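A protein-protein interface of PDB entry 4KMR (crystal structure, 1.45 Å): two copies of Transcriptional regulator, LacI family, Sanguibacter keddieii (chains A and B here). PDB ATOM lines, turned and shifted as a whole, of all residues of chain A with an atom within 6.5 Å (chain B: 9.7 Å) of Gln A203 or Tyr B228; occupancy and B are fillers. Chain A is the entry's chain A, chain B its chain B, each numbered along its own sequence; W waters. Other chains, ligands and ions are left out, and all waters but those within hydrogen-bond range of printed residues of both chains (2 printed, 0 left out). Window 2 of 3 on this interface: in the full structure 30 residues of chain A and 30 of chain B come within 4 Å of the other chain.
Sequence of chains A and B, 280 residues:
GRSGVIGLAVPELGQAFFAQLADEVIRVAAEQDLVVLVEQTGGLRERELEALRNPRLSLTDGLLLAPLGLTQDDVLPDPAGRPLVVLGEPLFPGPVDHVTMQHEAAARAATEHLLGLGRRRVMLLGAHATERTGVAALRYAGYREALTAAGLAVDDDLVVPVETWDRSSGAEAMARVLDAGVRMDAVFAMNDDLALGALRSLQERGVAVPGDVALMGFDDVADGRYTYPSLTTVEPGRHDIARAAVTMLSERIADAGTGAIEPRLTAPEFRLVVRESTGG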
ATOM      1  N   ALA A 198       8.697  -5.382  13.870  1.00  0.00           N
ATOM      2  CA  ALA A 198       7.461  -5.957  13.397  1.00  0.00           C
ATOM      3  C   ALA A 198       6.933  -6.992  14.360  1.00  0.00           C
ATOM      4  O   ALA A 198       5.738  -7.054  14.597  1.00  0.00           O
ATOM      5  CB  ALA A 198       7.641  -6.558  12.017  1.00  0.00           C
ATOM      6  N   LEU A 199       7.834  -7.826  14.883  1.00  0.00           N
ATOM      7  CA  LEU A 199       7.451  -8.852  15.842  1.00  0.00           C
ATOM      8  C   LEU A 199       6.700  -8.265  17.046  1.00  0.00           C
ATOM      9  O   LEU A 199       5.648  -8.791  17.458  1.00  0.00           O
ATOM     10  CB  LEU A 199       8.640  -9.673  16.315  1.00  0.00           C
ATOM     11  CG  LEU A 199       8.353 -10.841  17.286  1.00  0.00           C
ATOM     12  CD1 LEU A 199       7.379 -11.858  16.660  1.00  0.00           C
ATOM     13  CD2 LEU A 199       9.715 -11.460  17.712  1.00  0.00           C
ATOM     14  N   ARG A 200       7.210  -7.155  17.566  1.00  0.00           N
ATOM     15  CA  ARG A 200       6.537  -6.539  18.684  1.00  0.00           C
ATOM     16  C   ARG A 200       5.138  -6.112  18.306  1.00  0.00           C
ATOM     17  O   ARG A 200       4.189  -6.360  19.054  1.00  0.00           O
ATOM     18  CB  ARG A 200       7.252  -5.347  19.236  1.00  0.00           C
ATOM     19  CG  ARG A 200       6.395  -4.764  20.343  1.00  0.00           C
ATOM     20  CD  ARG A 200       7.030  -3.679  21.101  1.00  0.00           C
ATOM     21  NE  ARG A 200       5.925  -3.119  21.831  1.00  0.00           N
ATOM     22  CZ  ARG A 200       5.718  -3.225  23.129  1.00  0.00           C
ATOM     23  NH1 ARG A 200       6.613  -3.773  23.924  1.00  0.00           N
ATOM     24  NH2 ARG A 200       4.608  -2.687  23.651  1.00  0.00           N
ATOM     25  N   SER A 201       4.996  -5.460  17.154  1.00  0.00           N
ATOM     26  CA  SER A 201       3.661  -4.979  16.750  1.00  0.00           C
ATOM     27  C   SER A 201       2.696  -6.143  16.537  1.00  0.00           C
ATOM     28  O   SER A 201       1.519  -6.036  16.889  1.00  0.00           O
ATOM     29  CB  SER A 201       3.776  -4.096  15.530  1.00  0.00           C
ATOM     30  OG  SER A 201       4.451  -2.928  15.834  1.00  0.00           O
ATOM     31  N   LEU A 202       3.206  -7.274  16.011  1.00  0.00           N
ATOM     32  CA  LEU A 202       2.389  -8.466  15.829  1.00  0.00           C
ATOM     33  C   LEU A 202       1.967  -9.019  17.172  1.00  0.00           C
ATOM     34  O   LEU A 202       0.775  -9.319  17.405  1.00  0.00           O
ATOM     35  CB  LEU A 202       3.167  -9.520  15.047  1.00  0.00           C
ATOM     36  CG  LEU A 202       3.285  -9.264  13.529  1.00  0.00           C
ATOM     37  CD1 LEU A 202       4.492  -9.995  12.945  1.00  0.00           C
ATOM     38  CD2 LEU A 202       1.993  -9.630  12.805  1.00  0.00           C
ATOM     39  N   GLN A 203       2.924  -9.101  18.095  1.00  0.00           N
ATOM     40  CA  GLN A 203       2.602  -9.723  19.413  1.00  0.00           C
ATOM     41  C   GLN A 203       1.663  -8.897  20.242  1.00  0.00           C
ATOM     42  O   GLN A 203       0.772  -9.427  20.928  1.00  0.00           O
ATOM     43  CB  GLN A 203       3.876 -10.056  20.176  1.00  0.00           C
ATOM     44  CG  GLN A 203       4.639 -11.218  19.509  1.00  0.00           C
ATOM     45  CD  GLN A 203       5.978 -11.499  20.115  1.00  0.00           C
ATOM     46  OE1 GLN A 203       6.663 -10.605  20.604  1.00  0.00           O
ATOM     47  NE2 GLN A 203       6.374 -12.757  20.070  1.00  0.00           N
ATOM     48  N   GLU A 204       1.831  -7.587  20.140  1.00  0.00           N
ATOM     49  CA  GLU A 204       0.979  -6.669  20.916  1.00  0.00           C
ATOM     50  C   GLU A 204      -0.484  -6.695  20.431  1.00  0.00           C
ATOM     51  O   GLU A 204      -1.415  -6.323  21.163  1.00  0.00           O
ATOM     52  CB  GLU A 204       1.644  -5.269  21.013  1.00  0.00           C
ATOM     53  CG  GLU A 204       1.598  -4.388  19.814  1.00  0.00           C
ATOM     54  CD  GLU A 204       2.333  -3.036  19.988  1.00  0.00           C
ATOM     55  OE1 GLU A 204       2.293  -2.257  19.020  1.00  0.00           O
ATOM     56  OE2 GLU A 204       2.972  -2.729  21.029  1.00  0.00           O
ATOM     57  N   ARG A 205      -0.689  -7.166  19.200  1.00  0.00           N
ATOM     58  CA  ARG A 205      -2.022  -7.320  18.600  1.00  0.00           C
ATOM     59  C   ARG A 205      -2.580  -8.761  18.683  1.00  0.00           C
ATOM     60  O   ARG A 205      -3.657  -9.061  18.164  1.00  0.00           O
ATOM     61  CB  ARG A 205      -1.980  -6.839  17.158  1.00  0.00           C
ATOM     62  CG  ARG A 205      -1.925  -5.326  17.076  1.00  0.00           C
ATOM     63  CD  ARG A 205      -1.390  -4.802  15.765  1.00  0.00           C
ATOM     64  NE  ARG A 205      -1.458  -3.373  15.879  1.00  0.00           N
ATOM     65  CZ  ARG A 205      -0.630  -2.630  16.583  1.00  0.00           C
ATOM     66  NH1 ARG A 205       0.444  -3.165  17.144  1.00  0.00           N
ATOM     67  NH2 ARG A 205      -0.880  -1.332  16.703  1.00  0.00           N
ATOM     68  N   GLY A 206      -1.828  -9.623  19.368  1.00  0.00           N
ATOM     69  CA  GLY A 206      -2.182 -11.018  19.563  1.00  0.00           C
ATOM     70  C   GLY A 206      -2.095 -11.912  18.325  1.00  0.00           C
ATOM     71  O   GLY A 206      -2.798 -12.930  18.234  1.00  0.00           O
ATOM     72  N   VAL A 207      -1.261 -11.519  17.359  1.00  0.00           N
ATOM     73  CA  VAL A 207      -1.127 -12.274  16.137  1.00  0.00           C
ATOM     74  C   VAL A 207      -0.067 -13.354  16.381  1.00  0.00           C
ATOM     75  O   VAL A 207       1.048 -13.038  16.744  1.00  0.00           O
ATOM     76  CB  VAL A 207      -0.698 -11.346  14.978  1.00  0.00           C
ATOM     77  CG1 VAL A 207      -0.566 -12.127  13.692  1.00  0.00           C
ATOM     78  CG2 VAL A 207      -1.691 -10.218  14.816  1.00  0.00           C
ATOM     79  N   VAL A 209       2.848 -15.907  15.825  1.00  0.00           N
ATOM     80  CA  VAL A 209       4.001 -16.020  14.957  1.00  0.00           C
ATOM     81  C   VAL A 209       4.670 -17.351  15.323  1.00  0.00           C
ATOM     82  O   VAL A 209       5.177 -17.493  16.439  1.00  0.00           O
ATOM     83  CB  VAL A 209       4.984 -14.858  15.145  1.00  0.00           C
ATOM     84  CG1 VAL A 209       6.203 -15.012  14.222  1.00  0.00           C
ATOM     85  CG2 VAL A 209       4.315 -13.520  14.839  1.00  0.00           C
ATOM     86  N   TYR A 228      12.035 -14.570  21.034  1.00  0.00           N
ATOM     87  CA  TYR A 228      10.914 -15.467  21.210  1.00  0.00           C
ATOM     88  C   TYR A 228       9.683 -14.999  20.391  1.00  0.00           C
ATOM     89  O   TYR A 228       9.079 -13.949  20.678  1.00  0.00           O
ATOM     90  CB  TYR A 228      10.547 -15.637  22.679  1.00  0.00           C
ATOM     91  CG  TYR A 228       9.467 -16.650  22.864  1.00  0.00           C
ATOM     92  CD1 TYR A 228       9.769 -18.001  22.800  1.00  0.00           C
ATOM     93  CD2 TYR A 228       8.146 -16.276  23.027  1.00  0.00           C
ATOM     94  CE1 TYR A 228       8.786 -18.967  22.909  1.00  0.00           C
ATOM     95  CE2 TYR A 228       7.143 -17.243  23.176  1.00  0.00           C
ATOM     96  CZ  TYR A 228       7.471 -18.580  23.095  1.00  0.00           C
ATOM     97  OH  TYR A 228       6.497 -19.542  23.236  1.00  0.00           O
ATOM     98  N   PRO A 229       9.347 -15.756  19.336  1.00  0.00           N
ATOM     99  CA  PRO A 229      10.017 -16.939  18.802  1.00  0.00           C
ATOM    100  C   PRO A 229      11.434 -16.588  18.302  1.00  0.00           C
ATOM    101  O   PRO A 229      11.685 -15.401  17.942  1.00  0.00           O
ATOM    102  CB  PRO A 229       9.114 -17.327  17.625  1.00  0.00           C
ATOM    103  CG  PRO A 229       8.463 -16.061  17.205  1.00  0.00           C
ATOM    104  CD  PRO A 229       8.196 -15.369  18.501  1.00  0.00           C
ATOM    105  N   LEU B 196      17.754 -10.505  28.422  1.00  0.00           N
ATOM    106  CA  LEU B 196      17.042 -10.869  27.159  1.00  0.00           C
ATOM    107  C   LEU B 196      17.045 -12.421  26.967  1.00  0.00           C
ATOM    108  O   LEU B 196      16.033 -13.005  26.559  1.00  0.00           O
ATOM    109  CB  LEU B 196      17.689 -10.173  25.994  1.00  0.00           C
ATOM    110  CG  LEU B 196      17.471  -8.672  25.952  1.00  0.00           C
ATOM    111  CD1 LEU B 196      18.436  -7.948  25.006  1.00  0.00           C
ATOM    112  CD2 LEU B 196      16.062  -8.327  25.630  1.00  0.00           C
ATOM    113  N   LEU B 199      14.535 -13.780  29.432  1.00  0.00           N
ATOM    114  CA  LEU B 199      13.167 -13.522  28.976  1.00  0.00           C
ATOM    115  C   LEU B 199      12.701 -14.691  28.071  1.00  0.00           C
ATOM    116  O   LEU B 199      11.571 -15.159  28.185  1.00  0.00           O
ATOM    117  CB  LEU B 199      13.062 -12.136  28.310  1.00  0.00           C
ATOM    118  CG  LEU B 199      11.687 -11.778  27.806  1.00  0.00           C
ATOM    119  CD1 LEU B 199      10.674 -11.723  28.972  1.00  0.00           C
ATOM    120  CD2 LEU B 199      11.773 -10.475  27.048  1.00  0.00           C
ATOM    121  N   ARG B 200      13.530 -15.109  27.120  1.00  0.00           N
ATOM    122  CA  ARG B 200      13.162 -16.203  26.249  1.00  0.00           C
ATOM    123  C   ARG B 200      12.853 -17.463  27.069  1.00  0.00           C
ATOM    124  O   ARG B 200      11.841 -18.114  26.841  1.00  0.00           O
ATOM    125  CB  ARG B 200      14.262 -16.531  25.265  1.00  0.00           C
ATOM    126  CG  ARG B 200      13.983 -17.839  24.515  1.00  0.00           C
ATOM    127  CD  ARG B 200      14.927 -18.085  23.397  1.00  0.00           C
ATOM    128  NE  ARG B 200      14.749 -19.434  22.928  1.00  0.00           N
ATOM    129  CZ  ARG B 200      13.907 -19.829  21.963  1.00  0.00           C
ATOM    130  NH1 ARG B 200      13.158 -18.977  21.266  1.00  0.00           N
ATOM    131  NH2 ARG B 200      13.849 -21.125  21.688  1.00  0.00           N
ATOM    132  N   LEU B 202      11.841 -17.761  30.133  1.00  0.00           N
ATOM    133  CA  LEU B 202      10.579 -17.549  30.857  1.00  0.00           C
ATOM    134  C   LEU B 202       9.406 -17.700  29.877  1.00  0.00           C
ATOM    135  O   LEU B 202       8.441 -18.427  30.137  1.00  0.00           O
ATOM    136  CB  LEU B 202      10.588 -16.164  31.480  1.00  0.00           C
ATOM    137  CG  LEU B 202      11.521 -16.016  32.705  1.00  0.00           C
ATOM    138  CD1 LEU B 202      11.941 -14.580  32.972  1.00  0.00           C
ATOM    139  CD2 LEU B 202      10.808 -16.556  33.966  1.00  0.00           C
ATOM    140  N   GLN B 203       9.491 -17.032  28.732  1.00  0.00           N
ATOM    141  CA  GLN B 203       8.364 -17.043  27.760  1.00  0.00           C
ATOM    142  C   GLN B 203       8.112 -18.427  27.175  1.00  0.00           C
ATOM    143  O   GLN B 203       6.948 -18.847  27.000  1.00  0.00           O
ATOM    144  CB  GLN B 203       8.598 -16.019  26.631  1.00  0.00           C
ATOM    145  CG  GLN B 203       8.541 -14.566  27.071  1.00  0.00           C
ATOM    146  CD  GLN B 203       9.024 -13.618  25.975  1.00  0.00           C
ATOM    147  OE1 GLN B 203      10.060 -13.862  25.325  1.00  0.00           O
ATOM    148  NE2 GLN B 203       8.385 -12.502  25.875  1.00  0.00           N
ATOM    149  N   GLU B 204       9.189 -19.158  26.906  1.00  0.00           N
ATOM    150  CA  GLU B 204       9.016 -20.485  26.294  1.00  0.00           C
ATOM    151  C   GLU B 204       8.329 -21.497  27.235  1.00  0.00           C
ATOM    152  O   GLU B 204       7.769 -22.503  26.800  1.00  0.00           O
ATOM    153  CB  GLU B 204      10.278 -21.033  25.649  1.00  0.00           C
ATOM    154  CG  GLU B 204      11.324 -21.487  26.589  1.00  0.00           C
ATOM    155  CD  GLU B 204      12.633 -21.931  25.876  1.00  0.00           C
ATOM    156  OE1 GLU B 204      13.608 -22.053  26.616  1.00  0.00           O
ATOM    157  OE2 GLU B 204      12.736 -22.056  24.632  1.00  0.00           O
ATOM    158  N   VAL B 207       5.742 -18.521  31.439  1.00  0.00           N
ATOM    159  CA  VAL B 207       5.803 -17.757  32.678  1.00  0.00           C
ATOM    160  C   VAL B 207       5.527 -16.290  32.274  1.00  0.00           C
ATOM    161  O   VAL B 207       6.220 -15.728  31.431  1.00  0.00           O
ATOM    162  CB  VAL B 207       7.169 -17.901  33.412  1.00  0.00           C
ATOM    163  CG1 VAL B 207       7.218 -17.073  34.688  1.00  0.00           C
ATOM    164  CG2 VAL B 207       7.504 -19.374  33.699  1.00  0.00           C
ATOM    165  N   ALA B 208       4.514 -15.690  32.879  1.00  0.00           N
ATOM    166  CA  ALA B 208       4.122 -14.292  32.574  1.00  0.00           C
ATOM    167  C   ALA B 208       5.179 -13.311  33.160  1.00  0.00           C
ATOM    168  O   ALA B 208       5.613 -13.417  34.322  1.00  0.00           O
ATOM    169  CB  ALA B 208       2.735 -14.033  33.153  1.00  0.00           C
ATOM    170  N   VAL B 209       5.547 -12.332  32.338  1.00  0.00           N
ATOM    171  CA  VAL B 209       6.463 -11.267  32.722  1.00  0.00           C
ATOM    172  C   VAL B 209       5.691  -9.970  32.404  1.00  0.00           C
ATOM    173  O   VAL B 209       5.401  -9.693  31.226  1.00  0.00           O
ATOM    174  CB  VAL B 209       7.787 -11.299  31.930  1.00  0.00           C
ATOM    175  CG1 VAL B 209       8.683 -10.173  32.367  1.00  0.00           C
ATOM    176  CG2 VAL B 209       8.477 -12.648  32.133  1.00  0.00           C
ATOM    177  N   PRO B 210       5.400  -9.157  33.412  1.00  0.00           N
ATOM    178  CA  PRO B 210       5.771  -9.220  34.806  1.00  0.00           C
ATOM    179  C   PRO B 210       4.862  -9.989  35.738  1.00  0.00           C
ATOM    180  O   PRO B 210       5.176 -10.094  36.922  1.00  0.00           O
ATOM    181  CB  PRO B 210       5.712  -7.741  35.213  1.00  0.00           C
ATOM    182  CG  PRO B 210       4.571  -7.189  34.399  1.00  0.00           C
ATOM    183  CD  PRO B 210       4.647  -7.919  33.090  1.00  0.00           C
ATOM    184  N   LEU B 215      11.112  -8.611  35.603  1.00  0.00           N
ATOM    185  CA  LEU B 215      12.467  -8.751  35.095  1.00  0.00           C
ATOM    186  C   LEU B 215      13.101  -7.441  34.742  1.00  0.00           C
ATOM    187  O   LEU B 215      12.442  -6.586  34.151  1.00  0.00           O
ATOM    188  CB  LEU B 215      12.403  -9.635  33.787  1.00  0.00           C
ATOM    189  CG  LEU B 215      13.681  -9.839  32.990  1.00  0.00           C
ATOM    190  CD1 LEU B 215      14.704 -10.679  33.738  1.00  0.00           C
ATOM    191  CD2 LEU B 215      13.301 -10.471  31.643  1.00  0.00           C
ATOM    192  N   ASP B 223      17.848  -2.991  22.050  1.00  0.00           N
ATOM    193  CA  ASP B 223      16.922  -4.095  21.841  1.00  0.00           C
ATOM    194  C   ASP B 223      15.815  -4.184  22.898  1.00  0.00           C
ATOM    195  O   ASP B 223      14.702  -4.618  22.621  1.00  0.00           O
ATOM    196  CB  ASP B 223      17.702  -5.429  21.834  1.00  0.00           C
ATOM    197  CG  ASP B 223      18.994  -5.419  20.935  1.00  0.00           C
ATOM    198  OD1 ASP B 223      19.263  -6.499  20.359  1.00  0.00           O
ATOM    199  OD2 ASP B 223      19.746  -4.390  20.839  1.00  0.00           O
ATOM    200  N   GLY B 224      16.106  -3.727  24.106  1.00  0.00           N
ATOM    201  CA  GLY B 224      15.154  -3.815  25.214  1.00  0.00           C
ATOM    202  C   GLY B 224      13.891  -2.954  25.026  1.00  0.00           C
ATOM    203  O   GLY B 224      12.879  -3.164  25.705  1.00  0.00           O
ATOM    204  N   ARG B 225      13.947  -1.960  24.122  1.00  0.00           N
ATOM    205  CA  ARG B 225      12.743  -1.146  23.855  1.00  0.00           C
ATOM    206  C   ARG B 225      11.690  -1.915  23.058  1.00  0.00           C
ATOM    207  O   ARG B 225      10.519  -1.501  23.059  1.00  0.00           O
ATOM    208  CB  ARG B 225      13.104   0.103  23.058  1.00  0.00           C
ATOM    209  CG  ARG B 225      13.875   1.155  23.828  1.00  0.00           C
ATOM    210  CD  ARG B 225      14.245   2.330  22.927  1.00  0.00           C
ATOM    211  NE  ARG B 225      15.026   3.269  23.679  1.00  0.00           N
ATOM    212  CZ  ARG B 225      15.366   4.495  23.267  1.00  0.00           C
ATOM    213  NH1 ARG B 225      15.000   4.904  22.047  1.00  0.00           N
ATOM    214  NH2 ARG B 225      16.094   5.297  24.060  1.00  0.00           N
ATOM    215  N   TYR B 226      12.084  -3.007  22.353  1.00  0.00           N
ATOM    216  CA  TYR B 226      11.162  -3.663  21.427  1.00  0.00           C
ATOM    217  C   TYR B 226      10.815  -5.099  21.696  1.00  0.00           C
ATOM    218  O   TYR B 226      10.168  -5.740  20.870  1.00  0.00           O
ATOM    219  CB  TYR B 226      11.581  -3.409  19.956  1.00  0.00           C
ATOM    220  CG  TYR B 226      11.207  -2.021  19.593  1.00  0.00           C
ATOM    221  CD1 TYR B 226      12.136  -1.000  19.657  1.00  0.00           C
ATOM    222  CD2 TYR B 226       9.871  -1.710  19.301  1.00  0.00           C
ATOM    223  CE1 TYR B 226      11.747   0.324  19.381  1.00  0.00           C
ATOM    224  CE2 TYR B 226       9.449  -0.429  19.085  1.00  0.00           C
ATOM    225  CZ  TYR B 226      10.358   0.589  19.085  1.00  0.00           C
ATOM    226  OH  TYR B 226       9.815   1.834  18.833  1.00  0.00           O
ATOM    227  N   THR B 227      11.270  -5.622  22.818  1.00  0.00           N
ATOM    228  CA  THR B 227      10.756  -6.906  23.258  1.00  0.00           C
ATOM    229  C   THR B 227       9.306  -6.685  23.704  1.00  0.00           C
ATOM    230  O   THR B 227       8.867  -5.530  23.837  1.00  0.00           O
ATOM    231  CB  THR B 227      11.619  -7.491  24.407  1.00  0.00           C
ATOM    232  OG1 THR B 227      11.846  -6.527  25.432  1.00  0.00           O
ATOM    233  CG2 THR B 227      12.917  -7.973  23.815  1.00  0.00           C
ATOM    234  N   TYR B 228       8.584  -7.789  23.974  1.00  0.00           N
ATOM    235  CA  TYR B 228       7.182  -7.741  24.449  1.00  0.00           C
ATOM    236  C   TYR B 228       7.060  -8.767  25.570  1.00  0.00           C
ATOM    237  O   TYR B 228       6.937  -9.971  25.311  1.00  0.00           O
ATOM    238  CB  TYR B 228       6.184  -7.970  23.323  1.00  0.00           C
ATOM    239  CG  TYR B 228       4.736  -7.821  23.744  1.00  0.00           C
ATOM    240  CD1 TYR B 228       4.223  -6.605  24.105  1.00  0.00           C
ATOM    241  CD2 TYR B 228       3.883  -8.897  23.723  1.00  0.00           C
ATOM    242  CE1 TYR B 228       2.897  -6.466  24.501  1.00  0.00           C
ATOM    243  CE2 TYR B 228       2.579  -8.788  24.100  1.00  0.00           C
ATOM    244  CZ  TYR B 228       2.076  -7.561  24.484  1.00  0.00           C
ATOM    245  OH  TYR B 228       0.758  -7.437  24.863  1.00  0.00           O
ATOM    246  N   PRO B 229       7.183  -8.324  26.838  1.00  0.00           N
ATOM    247  CA  PRO B 229       7.302  -6.956  27.329  1.00  0.00           C
ATOM    248  C   PRO B 229       8.609  -6.247  27.021  1.00  0.00           C
ATOM    249  O   PRO B 229       9.661  -6.873  27.005  1.00  0.00           O
ATOM    250  CB  PRO B 229       7.164  -7.139  28.855  1.00  0.00           C
ATOM    251  CG  PRO B 229       7.774  -8.454  29.116  1.00  0.00           C
ATOM    252  CD  PRO B 229       7.325  -9.297  27.943  1.00  0.00           C
ATOM    253  N   SER B 230       8.547  -4.936  26.921  1.00  0.00           N
ATOM    254  CA  SER B 230       9.753  -4.107  26.835  1.00  0.00           C
ATOM    255  C   SER B 230      10.513  -4.229  28.173  1.00  0.00           C
ATOM    256  O   SER B 230       9.894  -4.425  29.210  1.00  0.00           O
ATOM    257  CB  SER B 230       9.369  -2.696  26.487  1.00  0.00           C
ATOM    258  OG  SER B 230       8.397  -2.157  27.336  1.00  0.00           O
ATOM    259  N   LEU B 231      11.840  -4.119  28.117  1.00  0.00           N
ATOM    260  CA  LEU B 231      12.677  -4.458  29.245  1.00  0.00           C
ATOM    261  C   LEU B 231      13.048  -3.270  30.152  1.00  0.00           C
ATOM    262  O   LEU B 231      13.733  -2.359  29.688  1.00  0.00           O
ATOM    263  CB  LEU B 231      13.970  -5.089  28.717  1.00  0.00           C
ATOM    264  CG  LEU B 231      15.043  -5.500  29.717  1.00  0.00           C
ATOM    265  CD1 LEU B 231      14.515  -6.622  30.588  1.00  0.00           C
ATOM    266  CD2 LEU B 231      16.378  -5.896  29.067  1.00  0.00           C
ATOM    267  N   THR B 232      12.680  -3.306  31.421  1.00  0.00           N
ATOM    268  CA  THR B 232      13.168  -2.306  32.398  1.00  0.00           C
ATOM    269  C   THR B 232      14.683  -2.525  32.544  1.00  0.00           C
ATOM    270  O   THR B 232      15.200  -3.647  32.528  1.00  0.00           O
ATOM    271  CB  THR B 232      12.447  -2.518  33.712  1.00  0.00           C
ATOM    272  OG1 THR B 232      11.063  -2.213  33.489  1.00  0.00           O
ATOM    273  CG2 THR B 232      13.004  -1.667  34.826  1.00  0.00           C
ATOM    274  N   ARG B 275      10.135   0.097  32.085  1.00  0.00           N
ATOM    275  CA  ARG B 275       9.395  -0.425  30.945  1.00  0.00           C
ATOM    276  C   ARG B 275       8.344  -1.463  31.388  1.00  0.00           C
ATOM    277  O   ARG B 275       8.039  -1.605  32.561  1.00  0.00           O
ATOM    278  CB  ARG B 275      10.309  -0.897  29.835  1.00  0.00           C
ATOM    279  CG  ARG B 275      11.378   0.124  29.448  1.00  0.00           C
ATOM    280  CD  ARG B 275      11.960  -0.103  28.076  1.00  0.00           C
ATOM    281  NE  ARG B 275      12.963   0.845  27.686  1.00  0.00           N
ATOM    282  CZ  ARG B 275      14.266   0.582  27.525  1.00  0.00           C
ATOM    283  NH1 ARG B 275      14.783  -0.630  27.692  1.00  0.00           N
ATOM    284  NH2 ARG B 275      15.051   1.552  27.092  1.00  0.00           N
ATOM    285  N   GLU B 276       7.812  -2.218  30.448  1.00  0.00           N
ATOM    286  CA  GLU B 276       6.695  -3.114  30.749  1.00  0.00           C
ATOM    287  C   GLU B 276       7.063  -4.324  31.619  1.00  0.00           C
ATOM    288  O   GLU B 276       6.238  -4.866  32.333  1.00  0.00           O
ATOM    289  CB  GLU B 276       6.103  -3.635  29.454  1.00  0.00           C
ATOM    290  CG  GLU B 276       5.398  -2.602  28.581  1.00  0.00           C
ATOM    291  CD  GLU B 276       5.124  -3.086  27.141  1.00  0.00           C
ATOM    292  OE1 GLU B 276       5.750  -4.056  26.665  1.00  0.00           O
ATOM    293  OE2 GLU B 276       4.274  -2.454  26.464  1.00  0.00           O
ATOM    294  N   SER B 277       8.335  -4.714  31.598  1.00  0.00           N
ATOM    295  CA  SER B 277       8.757  -5.958  32.294  1.00  0.00           C
ATOM    296  C   SER B 277       8.759  -5.872  33.801  1.00  0.00           C
ATOM    297  O   SER B 277       8.917  -6.902  34.437  1.00  0.00           O
ATOM    298  CB  SER B 277      10.064  -6.478  31.752  1.00  0.00           C
ATOM    299  OG  SER B 277      11.144  -5.650  32.111  1.00  0.00           O
HETATM  300  O   HOH W   1       6.133 -11.727  23.345  1.00  0.00           O
HETATM  301  O   HOH W   2       7.159 -22.650  24.103  1.00  0.00           O
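Water W1 lies within hydrogen-bond range of the backbone carbonyl oxygen of Tyr B228 (2.8 Å), the side-chain amide oxygen of Gln A203 (3.0 Å) and the side-chain amide nitrogen of Gln B203 (3.5 Å). Water W2 bridges the backbone carbonyl oxygen of Glu B204 and the side-chain hydroxyl of Tyr A228.
Among the printed residues, Asp or Glu carboxylates within 4 Å of a Lys or Arg side-chain nitrogen of the other chain: Arg A200 with Glu B276.
The guanidinium group (NH2) of Arg B200 lies within salt-bridge range of the side-chain carboxylate (OE2) of Glu B204. The side-chain amide nitrogen of Gln B203 sits at hydrogen-bond distance from the backbone carbonyl oxygen of Tyr B228. OG1 of Thr B227 is in hydrogen-bond range of O of Pro B229, 2.7 Å away. The backbone NH (N) of Ser B230 lies within hydrogen-bond range of the side-chain carboxylate (OE1) of Glu B276, 2.9 Å away. OE2 of Glu A204 lies within salt-bridge range of NE of Arg A200 (3.1 Å). The backbone carbonyl oxygen (O) of Ser B230 is in hydrogen-bond range of the backbone NH (N) of Ser B277, at 2.9 Å.
Arg A200 touches Tyr B228, and with the chains exchanged Tyr A228 touches Arg B200. Gln A203 touches Tyr B228, and with the chains exchanged Tyr A228 touches Gln B203. Glu A204 touches Tyr B228, and with the chains exchanged Tyr A228 touches Glu B204.
NH2 of Arg A200 lies within salt-bridge range of OE2 of Glu B276, at 2.8 Å. NH1 of Arg A200 lies within hydrogen-bond range of O of Thr B227 (2.9 Å).
Among the printed residues, merely in contact across the chains: Tyr A228 with Gln B203, Arg A200 with Tyr B226, Gln A203 with Tyr B228, Arg A200 with Tyr B228, Tyr A228 with Glu B204, Arg A200 with Ser B230, Glu A204 with Tyr B228 and Tyr A228 with Arg B200.
Of chain B, only Tyr B228 comes within 4 Å of Gln A203. Of chain A, only Arg A200 (3.7 Å), Gln A203 (3.7 Å) and Glu A204 (3.8 Å) come within 4 Å of Tyr B228. Arg A200 touches just these residues of chain B: Tyr B226 (3.4 Å), Thr B227 (2.9 Å), Tyr B228 (3.7 Å), Ser B230 (3.8 Å) and Glu B276 (2.8 Å). Printed residues of chain B within 4 Å of Tyr A228: Arg B200 (3.8 Å), Gln B203 (3.2 Å) and Glu B204 (3.7 Å). Printed residues of chain A within 4 Å of Thr B227: Arg A200.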
